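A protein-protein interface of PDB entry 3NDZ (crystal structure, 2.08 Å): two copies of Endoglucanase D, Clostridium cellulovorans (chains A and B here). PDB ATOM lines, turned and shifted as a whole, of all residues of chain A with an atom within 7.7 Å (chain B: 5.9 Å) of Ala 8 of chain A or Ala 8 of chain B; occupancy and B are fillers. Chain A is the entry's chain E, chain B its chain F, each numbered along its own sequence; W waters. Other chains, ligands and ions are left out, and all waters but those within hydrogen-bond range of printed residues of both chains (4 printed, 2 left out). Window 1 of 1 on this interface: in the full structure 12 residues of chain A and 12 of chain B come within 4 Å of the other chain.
O of Thr 10 of chain B lies within hydrogen-bond range of NZ of Lys 93 of chain A (2.8 Å). The side-chain amide oxygen of Asn 20 of chain B is in hydrogen-bond range of the side-chain hydroxyl of Thr 22 of chain A (3.1 Å). The side-chain amino group (NZ) of Lys 93 of chain B sits at hydrogen-bond distance from the backbone carbonyl oxygen (O) of Thr 10 of chain A (3.2 Å). O of Ile 9 of chain A lies within hydrogen-bond range of N of Ile 9 of chain B.
Among the printed residues, pairs that only touch across the chains: Thr 6 of chain A with Thr 10 of chain B (3.4 Å), Thr 6 of chain A with Asn 20 of chain B (3.9 Å), Tyr 7 of chain A with Thr 10 of chain B (3.8 Å), Ala 8 of chain A with Ala 8 of chain B (3.4 Å), Ala 8 of chain A with Ile 9 of chain B (3.4 Å), Ala 8 of chain A with Thr 10 of chain B (3.6 Å), Ile 9 of chain A with Ala 8 of chain B (3.5 Å), Ile 9 of chain A with Lys 93 of chain B (3.97 Å), Thr 10 of chain A with Thr 6 of chain B (3.4 Å), Thr 10 of chain A with Tyr 7 of chain B (3.9 Å), Thr 10 of chain A with Ala 8 of chain B (3.7 Å), Asn 20 of chain A with Thr 6 of chain B (3.8 Å), Asn 20 of chain A with Asn 20 of chain B (3.97 Å) and Lys 93 of chain A with Ile 9 of chain B (3.8 Å).
Water W3 bridges the side-chain amino group of Lys 93 of chain A and the backbone carbonyl oxygen of Ile 9 of chain B. Water W4 bridges NZ of Lys 93 of chain B and O of Ile 9 of chain A. Water W2 bridges the backbone carbonyl oxygen (O) of Tyr 7 of chain B and the backbone carbonyl oxygen (O) of Thr 10 of chain A. Water W1 bridges the backbone carbonyl oxygen (O) of Thr 10 of chain B and the backbone carbonyl oxygen (O) of Tyr 7 of chain A.
Printed residues of chain B within 4 Å of Ala 8 of chain A: Ala 8, Ile 9 and Thr 10. Ala 8 of chain B touches just these residues of chain A: Ala 8, Ile 9 and Thr 10. Printed residues of chain A within 4 Å of Thr 6 of chain B: Thr 10 and Asn 20. Of the printed residues of chain B, Asn 20 of chain A touches Thr 6 and Asn 20. Val 5 of chain A touches none of the printed residues of chain B. The nearest residue of chain B that does not touch Ala 8 of chain A is Asn 20 of chain B (4.3 Å). The nearest printed residue of chain B that does not touch Tyr 7 of chain A is Ile 9 of chain B (4.6 Å).
Ala 8 of chain A touches Ile 9 of chain B, and with the chains exchanged Ile 9 of chain A touches Ala 8 of chain B. Ala 8 of chain A touches Thr 10 of chain B, and with the chains exchanged Thr 10 of chain A touches Ala 8 of chain B. Thr 10 of chain A touches Lys 93 of chain B, and with the chains exchanged Lys 93 of chain A touches Thr 10 of chain B. Asn 20 of chain A touches its own counterpart, Asn 20 of chain B. 10 positions are printed for both chains. Of the 18 pairs that touch across the chains among the printed residues, 17 have their exchanged pair printed and touching as well.
Hydrophobic or aromatic side chains of chain A that line the printed part of chain B: Ala 8 and Ile 9. Along chain A the printed residues that touch a printed residue of chain B span positions 6 to 93. Hydrophobic or aromatic side chains of chain B that line the printed part of chain A: Ala 8 and Ile 9.
The backbone carbonyl oxygen (O) of Ala 8 of chain A sits at hydrogen-bond distance from the backbone NH (N) of Asn 20 of chain A, at 2.9 Å. The backbone NH (N) of Thr 10 of chain B sits at hydrogen-bond distance from the backbone carbonyl oxygen (O) of Ser 18 of chain B, 2.8 Å away. The backbone carbonyl oxygen (O) of Ala 8 of chain B is in hydrogen-bond range of the backbone NH (N) of Asn 20 of chain B. The backbone carbonyl oxygen of Thr 22 of chain A lies within hydrogen-bond range of the backbone NH of Thr 6 of chain A, at 2.8 Å. N of Thr 10 of chain A is in hydrogen-bond range of O of Ser 18 of chain A (2.8 Å). The backbone carbonyl oxygen of Phe 81 of chain A is in hydrogen-bond range of the side-chain amide nitrogen of Asn 20 of chain A, at 3.4 Å.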
ATOM      1  N   VAL A   5      -9.895 -10.518  19.326  1.00  0.00           N
ATOM      2  CA  VAL A   5      -9.669  -9.117  19.017  1.00  0.00           C
ATOM      3  C   VAL A   5     -10.228  -8.269  20.147  1.00  0.00           C
ATOM      4  O   VAL A   5     -11.391  -8.417  20.517  1.00  0.00           O
ATOM      5  CB  VAL A   5     -10.332  -8.714  17.691  1.00  0.00           C
ATOM      6  CG1 VAL A   5     -10.299  -7.194  17.513  1.00  0.00           C
ATOM      7  CG2 VAL A   5      -9.663  -9.427  16.517  1.00  0.00           C
ATOM      8  N   THR A   6      -9.386  -7.398  20.701  1.00  0.00           N
ATOM      9  CA  THR A   6      -9.810  -6.456  21.728  1.00  0.00           C
ATOM     10  C   THR A   6      -9.857  -5.051  21.146  1.00  0.00           C
ATOM     11  O   THR A   6      -8.834  -4.508  20.735  1.00  0.00           O
ATOM     12  CB  THR A   6      -8.868  -6.466  22.928  1.00  0.00           C
ATOM     13  OG1 THR A   6      -8.891  -7.761  23.530  1.00  0.00           O
ATOM     14  CG2 THR A   6      -9.311  -5.432  23.960  1.00  0.00           C
ATOM     15  N   TYR A   7     -11.054  -4.475  21.108  1.00  0.00           N
ATOM     16  CA  TYR A   7     -11.283  -3.161  20.516  1.00  0.00           C
ATOM     17  C   TYR A   7     -11.639  -2.217  21.666  1.00  0.00           C
ATOM     18  O   TYR A   7     -12.692  -2.361  22.284  1.00  0.00           O
ATOM     19  CB  TYR A   7     -12.452  -3.277  19.546  1.00  0.00           C
ATOM     20  CG  TYR A   7     -12.687  -2.114  18.608  1.00  0.00           C
ATOM     21  CD1 TYR A   7     -13.353  -0.968  19.032  1.00  0.00           C
ATOM     22  CD2 TYR A   7     -12.300  -2.192  17.272  1.00  0.00           C
ATOM     23  CE1 TYR A   7     -13.595   0.080  18.160  1.00  0.00           C
ATOM     24  CE2 TYR A   7     -12.536  -1.153  16.396  1.00  0.00           C
ATOM     25  CZ  TYR A   7     -13.183  -0.022  16.842  1.00  0.00           C
ATOM     26  OH  TYR A   7     -13.421   1.002  15.962  1.00  0.00           O
ATOM     27  N   ALA A   8     -10.760  -1.266  21.963  1.00  0.00           N
ATOM     28  CA  ALA A   8     -10.911  -0.446  23.165  1.00  0.00           C
ATOM     29  C   ALA A   8     -10.774   1.041  22.893  1.00  0.00           C
ATOM     30  O   ALA A   8     -10.048   1.461  21.996  1.00  0.00           O
ATOM     31  CB  ALA A   8      -9.917  -0.876  24.235  1.00  0.00           C
ATOM     32  N   ILE A   9     -11.475   1.836  23.692  1.00  0.00           N
ATOM     33  CA  ILE A   9     -11.481   3.274  23.505  1.00  0.00           C
ATOM     34  C   ILE A   9     -10.490   3.946  24.436  1.00  0.00           C
ATOM     35  O   ILE A   9     -10.635   3.914  25.659  1.00  0.00           O
ATOM     36  CB  ILE A   9     -12.881   3.859  23.745  1.00  0.00           C
ATOM     37  CG1 ILE A   9     -13.874   3.247  22.759  1.00  0.00           C
ATOM     38  CG2 ILE A   9     -12.851   5.356  23.602  1.00  0.00           C
ATOM     39  CD1 ILE A   9     -13.362   3.259  21.334  1.00  0.00           C
ATOM     40  N   THR A  10      -9.475   4.552  23.846  1.00  0.00           N
ATOM     41  CA  THR A  10      -8.440   5.224  24.612  1.00  0.00           C
ATOM     42  C   THR A  10      -8.941   6.571  25.147  1.00  0.00           C
ATOM     43  O   THR A  10      -8.675   6.942  26.289  1.00  0.00           O
ATOM     44  CB  THR A  10      -7.189   5.440  23.738  1.00  0.00           C
ATOM     45  OG1 THR A  10      -6.704   4.166  23.288  1.00  0.00           O
ATOM     46  CG2 THR A  10      -6.107   6.142  24.518  1.00  0.00           C
ATOM     47  N   ASN A  11      -9.691   7.283  24.314  1.00  0.00           N
ATOM     48  CA  ASN A  11     -10.083   8.649  24.604  1.00  0.00           C
ATOM     49  C   ASN A  11     -11.197   9.017  23.635  1.00  0.00           C
ATOM     50  O   ASN A  11     -11.250   8.484  22.530  1.00  0.00           O
ATOM     51  CB  ASN A  11      -8.863   9.561  24.412  1.00  0.00           C
ATOM     52  CG  ASN A  11      -9.140  11.008  24.751  1.00  0.00           C
ATOM     53  OD1 ASN A  11     -10.066  11.327  25.499  1.00  0.00           O
ATOM     54  ND2 ASN A  11      -8.319  11.900  24.209  1.00  0.00           N
ATOM     55  N   SER A  18     -10.280   7.994  19.968  1.00  0.00           N
ATOM     56  CA  SER A  18      -9.048   7.307  19.666  1.00  0.00           C
ATOM     57  C   SER A  18      -9.184   5.853  20.098  1.00  0.00           C
ATOM     58  O   SER A  18      -9.598   5.566  21.229  1.00  0.00           O
ATOM     59  CB  SER A  18      -7.887   7.987  20.383  1.00  0.00           C
ATOM     60  OG  SER A  18      -6.698   7.245  20.197  1.00  0.00           O
ATOM     61  N   VAL A  19      -8.856   4.939  19.187  1.00  0.00           N
ATOM     62  CA  VAL A  19      -9.068   3.512  19.412  1.00  0.00           C
ATOM     63  C   VAL A  19      -7.738   2.777  19.459  1.00  0.00           C
ATOM     64  O   VAL A  19      -6.796   3.133  18.759  1.00  0.00           O
ATOM     65  CB  VAL A  19      -9.940   2.887  18.308  1.00  0.00           C
ATOM     66  CG1 VAL A  19     -10.275   1.426  18.631  1.00  0.00           C
ATOM     67  CG2 VAL A  19     -11.219   3.684  18.134  1.00  0.00           C
ATOM     68  N   ASN A  20      -7.668   1.780  20.326  1.00  0.00           N
ATOM     69  CA  ASN A  20      -6.545   0.871  20.364  1.00  0.00           C
ATOM     70  C   ASN A  20      -7.082  -0.530  20.138  1.00  0.00           C
ATOM     71  O   ASN A  20      -8.050  -0.957  20.793  1.00  0.00           O
ATOM     72  CB  ASN A  20      -5.803   0.968  21.705  1.00  0.00           C
ATOM     73  CG  ASN A  20      -4.482   0.197  21.704  1.00  0.00           C
ATOM     74  OD1 ASN A  20      -4.389  -0.886  22.274  1.00  0.00           O
ATOM     75  ND2 ASN A  20      -3.464   0.751  21.049  1.00  0.00           N
ATOM     76  N   VAL A  21      -6.477  -1.237  19.192  1.00  0.00           N
ATOM     77  CA  VAL A  21      -6.863  -2.623  18.902  1.00  0.00           C
ATOM     78  C   VAL A  21      -5.711  -3.578  19.216  1.00  0.00           C
ATOM     79  O   VAL A  21      -4.566  -3.339  18.830  1.00  0.00           O
ATOM     80  CB  VAL A  21      -7.284  -2.817  17.419  1.00  0.00           C
ATOM     81  CG1 VAL A  21      -7.675  -4.266  17.157  1.00  0.00           C
ATOM     82  CG2 VAL A  21      -8.442  -1.883  17.046  1.00  0.00           C
ATOM     83  N   THR A  22      -6.024  -4.657  19.919  1.00  0.00           N
ATOM     84  CA  THR A  22      -5.049  -5.691  20.213  1.00  0.00           C
ATOM     85  C   THR A  22      -5.554  -7.022  19.681  1.00  0.00           C
ATOM     86  O   THR A  22      -6.667  -7.458  20.004  1.00  0.00           O
ATOM     87  CB  THR A  22      -4.804  -5.817  21.726  1.00  0.00           C
ATOM     88  OG1 THR A  22      -4.261  -4.585  22.216  1.00  0.00           O
ATOM     89  CG2 THR A  22      -3.833  -6.973  22.037  1.00  0.00           C
ATOM     90  N   PHE A  81      -2.344  -1.902  17.305  1.00  0.00           N
ATOM     91  CA  PHE A  81      -2.228  -0.707  16.490  1.00  0.00           C
ATOM     92  C   PHE A  81      -3.331   0.217  16.988  1.00  0.00           C
ATOM     93  O   PHE A  81      -4.145  -0.188  17.810  1.00  0.00           O
ATOM     94  CB  PHE A  81      -2.384  -1.042  14.994  1.00  0.00           C
ATOM     95  CG  PHE A  81      -3.754  -1.560  14.621  1.00  0.00           C
ATOM     96  CD1 PHE A  81      -4.726  -0.699  14.115  1.00  0.00           C
ATOM     97  CD2 PHE A  81      -4.069  -2.894  14.771  1.00  0.00           C
ATOM     98  CE1 PHE A  81      -5.991  -1.171  13.779  1.00  0.00           C
ATOM     99  CE2 PHE A  81      -5.331  -3.374  14.451  1.00  0.00           C
ATOM    100  CZ  PHE A  81      -6.296  -2.511  13.952  1.00  0.00           C
ATOM    101  N   GLY A  82      -3.366   1.454  16.519  1.00  0.00           N
ATOM    102  CA  GLY A  82      -4.403   2.368  16.979  1.00  0.00           C
ATOM    103  C   GLY A  82      -4.792   3.319  15.877  1.00  0.00           C
ATOM    104  O   GLY A  82      -4.112   3.376  14.857  1.00  0.00           O
ATOM    105  N   PHE A  83      -5.884   4.057  16.077  1.00  0.00           N
ATOM    106  CA  PHE A  83      -6.324   5.059  15.113  1.00  0.00           C
ATOM    107  C   PHE A  83      -7.302   6.047  15.742  1.00  0.00           C
ATOM    108  O   PHE A  83      -7.916   5.749  16.769  1.00  0.00           O
ATOM    109  CB  PHE A  83      -6.972   4.394  13.887  1.00  0.00           C
ATOM    110  CG  PHE A  83      -8.134   3.489  14.219  1.00  0.00           C
ATOM    111  CD1 PHE A  83      -7.935   2.134  14.448  1.00  0.00           C
ATOM    112  CD2 PHE A  83      -9.429   3.987  14.284  1.00  0.00           C
ATOM    113  CE1 PHE A  83      -9.000   1.297  14.748  1.00  0.00           C
ATOM    114  CE2 PHE A  83     -10.498   3.158  14.585  1.00  0.00           C
ATOM    115  CZ  PHE A  83     -10.288   1.813  14.814  1.00  0.00           C
ATOM    116  N   LEU A  91     -21.114   6.115  20.008  1.00  0.00           N
ATOM    117  CA  LEU A  91     -19.871   5.462  19.600  1.00  0.00           C
ATOM    118  C   LEU A  91     -20.008   3.937  19.554  1.00  0.00           C
ATOM    119  O   LEU A  91     -19.751   3.253  20.546  1.00  0.00           O
ATOM    120  CB  LEU A  91     -18.735   5.859  20.543  1.00  0.00           C
ATOM    121  CG  LEU A  91     -17.356   5.272  20.246  1.00  0.00           C
ATOM    122  CD1 LEU A  91     -16.992   5.531  18.805  1.00  0.00           C
ATOM    123  CD2 LEU A  91     -16.316   5.861  21.179  1.00  0.00           C
ATOM    124  N   LYS A  93     -19.194  -0.019  18.216  1.00  0.00           N
ATOM    125  CA  LYS A  93     -17.994  -0.814  17.980  1.00  0.00           C
ATOM    126  C   LYS A  93     -18.306  -1.940  17.021  1.00  0.00           C
ATOM    127  O   LYS A  93     -19.352  -2.576  17.137  1.00  0.00           O
ATOM    128  CB  LYS A  93     -17.479  -1.387  19.297  1.00  0.00           C
ATOM    129  CG  LYS A  93     -17.469  -0.343  20.391  1.00  0.00           C
ATOM    130  CD  LYS A  93     -16.585  -0.710  21.557  1.00  0.00           C
ATOM    131  CE  LYS A  93     -16.690   0.373  22.628  1.00  0.00           C
ATOM    132  NZ  LYS A  93     -16.005  -0.030  23.882  1.00  0.00           N
ATOM    133  N   PHE A  97     -14.780  -9.523  13.604  1.00  0.00           N
ATOM    134  CA  PHE A  97     -13.498  -9.237  13.001  1.00  0.00           C
ATOM    135  C   PHE A  97     -13.002 -10.489  12.321  1.00  0.00           C
ATOM    136  O   PHE A  97     -13.241 -11.597  12.799  1.00  0.00           O
ATOM    137  CB  PHE A  97     -12.491  -8.804  14.058  1.00  0.00           C
ATOM    138  CG  PHE A  97     -12.888  -7.566  14.809  1.00  0.00           C
ATOM    139  CD1 PHE A  97     -13.626  -7.658  15.982  1.00  0.00           C
ATOM    140  CD2 PHE A  97     -12.505  -6.313  14.355  1.00  0.00           C
ATOM    141  CE1 PHE A  97     -13.993  -6.519  16.686  1.00  0.00           C
ATOM    142  CE2 PHE A  97     -12.865  -5.167  15.052  1.00  0.00           C
ATOM    143  CZ  PHE A  97     -13.609  -5.270  16.220  1.00  0.00           C
ATOM    144  N   THR B   6      -0.627   2.876  26.422  1.00  0.00           N
ATOM    145  CA  THR B   6      -2.002   3.096  26.008  1.00  0.00           C
ATOM    146  C   THR B   6      -2.957   2.373  26.953  1.00  0.00           C
ATOM    147  O   THR B   6      -2.935   1.144  27.080  1.00  0.00           O
ATOM    148  CB  THR B   6      -2.239   2.637  24.556  1.00  0.00           C
ATOM    149  OG1 THR B   6      -1.316   3.308  23.693  1.00  0.00           O
ATOM    150  CG2 THR B   6      -3.655   2.975  24.117  1.00  0.00           C
ATOM    151  N   TYR B   7      -3.785   3.159  27.623  1.00  0.00           N
ATOM    152  CA  TYR B   7      -4.724   2.667  28.616  1.00  0.00           C
ATOM    153  C   TYR B   7      -6.113   2.901  28.039  1.00  0.00           C
ATOM    154  O   TYR B   7      -6.536   4.042  27.885  1.00  0.00           O
ATOM    155  CB  TYR B   7      -4.545   3.481  29.896  1.00  0.00           C
ATOM    156  CG  TYR B   7      -5.259   2.964  31.124  1.00  0.00           C
ATOM    157  CD1 TYR B   7      -6.614   3.211  31.322  1.00  0.00           C
ATOM    158  CD2 TYR B   7      -4.565   2.273  32.114  1.00  0.00           C
ATOM    159  CE1 TYR B   7      -7.267   2.762  32.465  1.00  0.00           C
ATOM    160  CE2 TYR B   7      -5.208   1.822  33.263  1.00  0.00           C
ATOM    161  CZ  TYR B   7      -6.558   2.073  33.432  1.00  0.00           C
ATOM    162  OH  TYR B   7      -7.200   1.629  34.571  1.00  0.00           O
ATOM    163  N   ALA B   8      -6.815   1.825  27.709  1.00  0.00           N
ATOM    164  CA  ALA B   8      -8.046   1.940  26.933  1.00  0.00           C
ATOM    165  C   ALA B   8      -9.213   1.184  27.564  1.00  0.00           C
ATOM    166  O   ALA B   8      -9.012   0.172  28.225  1.00  0.00           O
ATOM    167  CB  ALA B   8      -7.806   1.440  25.537  1.00  0.00           C
ATOM    168  N   ILE B   9     -10.429   1.666  27.336  1.00  0.00           N
ATOM    169  CA  ILE B   9     -11.617   1.008  27.874  1.00  0.00           C
ATOM    170  C   ILE B   9     -12.276   0.083  26.850  1.00  0.00           C
ATOM    171  O   ILE B   9     -12.813   0.522  25.830  1.00  0.00           O
ATOM    172  CB  ILE B   9     -12.653   2.022  28.403  1.00  0.00           C
ATOM    173  CG1 ILE B   9     -11.994   2.986  29.384  1.00  0.00           C
ATOM    174  CG2 ILE B   9     -13.830   1.289  29.072  1.00  0.00           C
ATOM    175  CD1 ILE B   9     -11.410   2.295  30.597  1.00  0.00           C
ATOM    176  N   THR B  10     -12.224  -1.209  27.129  1.00  0.00           N
ATOM    177  CA  THR B  10     -12.794  -2.189  26.226  1.00  0.00           C
ATOM    178  C   THR B  10     -14.315  -2.149  26.315  1.00  0.00           C
ATOM    179  O   THR B  10     -15.018  -2.235  25.305  1.00  0.00           O
ATOM    180  CB  THR B  10     -12.300  -3.581  26.585  1.00  0.00           C
ATOM    181  OG1 THR B  10     -10.881  -3.629  26.397  1.00  0.00           O
ATOM    182  CG2 THR B  10     -12.974  -4.626  25.717  1.00  0.00           C
ATOM    183  N   SER B  18     -13.981  -2.980  31.742  1.00  0.00           N
ATOM    184  CA  SER B  18     -12.909  -3.832  31.284  1.00  0.00           C
ATOM    185  C   SER B  18     -11.859  -2.952  30.616  1.00  0.00           C
ATOM    186  O   SER B  18     -12.186  -2.134  29.763  1.00  0.00           O
ATOM    187  CB  SER B  18     -13.444  -4.888  30.316  1.00  0.00           C
ATOM    188  OG  SER B  18     -12.406  -5.762  29.913  1.00  0.00           O
ATOM    189  N   VAL B  19     -10.604  -3.129  31.010  1.00  0.00           N
ATOM    190  CA  VAL B  19      -9.522  -2.267  30.548  1.00  0.00           C
ATOM    191  C   VAL B  19      -8.510  -3.054  29.724  1.00  0.00           C
ATOM    192  O   VAL B  19      -8.191  -4.187  30.048  1.00  0.00           O
ATOM    193  CB  VAL B  19      -8.782  -1.639  31.752  1.00  0.00           C
ATOM    194  CG1 VAL B  19      -7.617  -0.765  31.284  1.00  0.00           C
ATOM    195  CG2 VAL B  19      -9.762  -0.835  32.625  1.00  0.00           C
ATOM    196  N   ASN B  20      -7.998  -2.446  28.662  1.00  0.00           N
ATOM    197  CA  ASN B  20      -6.867  -3.021  27.953  1.00  0.00           C
ATOM    198  C   ASN B  20      -5.673  -2.075  28.016  1.00  0.00           C
ATOM    199  O   ASN B  20      -5.805  -0.895  27.690  1.00  0.00           O
ATOM    200  CB  ASN B  20      -7.216  -3.297  26.491  1.00  0.00           C
ATOM    201  CG  ASN B  20      -6.136  -4.137  25.785  1.00  0.00           C
ATOM    202  OD1 ASN B  20      -5.360  -3.630  24.979  1.00  0.00           O
ATOM    203  ND2 ASN B  20      -6.076  -5.417  26.116  1.00  0.00           N
ATOM    204  N   VAL B  21      -4.516  -2.588  28.427  1.00  0.00           N
ATOM    205  CA  VAL B  21      -3.292  -1.781  28.502  1.00  0.00           C
ATOM    206  C   VAL B  21      -2.209  -2.304  27.553  1.00  0.00           C
ATOM    207  O   VAL B  21      -1.871  -3.478  27.593  1.00  0.00           O
ATOM    208  CB  VAL B  21      -2.697  -1.752  29.924  1.00  0.00           C
ATOM    209  CG1 VAL B  21      -1.361  -0.996  29.936  1.00  0.00           C
ATOM    210  CG2 VAL B  21      -3.685  -1.143  30.921  1.00  0.00           C
ATOM    211  N   LYS B  93      -8.955   7.665  34.149  1.00  0.00           N
ATOM    212  CA  LYS B  93      -7.777   6.828  33.942  1.00  0.00           C
ATOM    213  C   LYS B  93      -6.560   7.413  34.640  1.00  0.00           C
ATOM    214  O   LYS B  93      -6.536   8.604  34.950  1.00  0.00           O
ATOM    215  CB  LYS B  93      -7.478   6.612  32.458  1.00  0.00           C
ATOM    216  CG  LYS B  93      -8.324   7.398  31.511  1.00  0.00           C
ATOM    217  CD  LYS B  93      -8.897   6.494  30.443  1.00  0.00           C
ATOM    218  CE  LYS B  93      -9.766   7.297  29.490  1.00  0.00           C
ATOM    219  NZ  LYS B  93     -10.696   6.437  28.730  1.00  0.00           N
HETATM  220  O   HOH W   1     -15.371  -3.792  22.841  1.00  0.00           O
HETATM  221  O   HOH W   2      -6.182   6.848  28.183  1.00  0.00           O
HETATM  222  O   HOH W   3     -15.438   1.580  25.707  1.00  0.00           O
HETATM  223  O   HOH W   4     -12.268   5.739  26.809  1.00  0.00           O
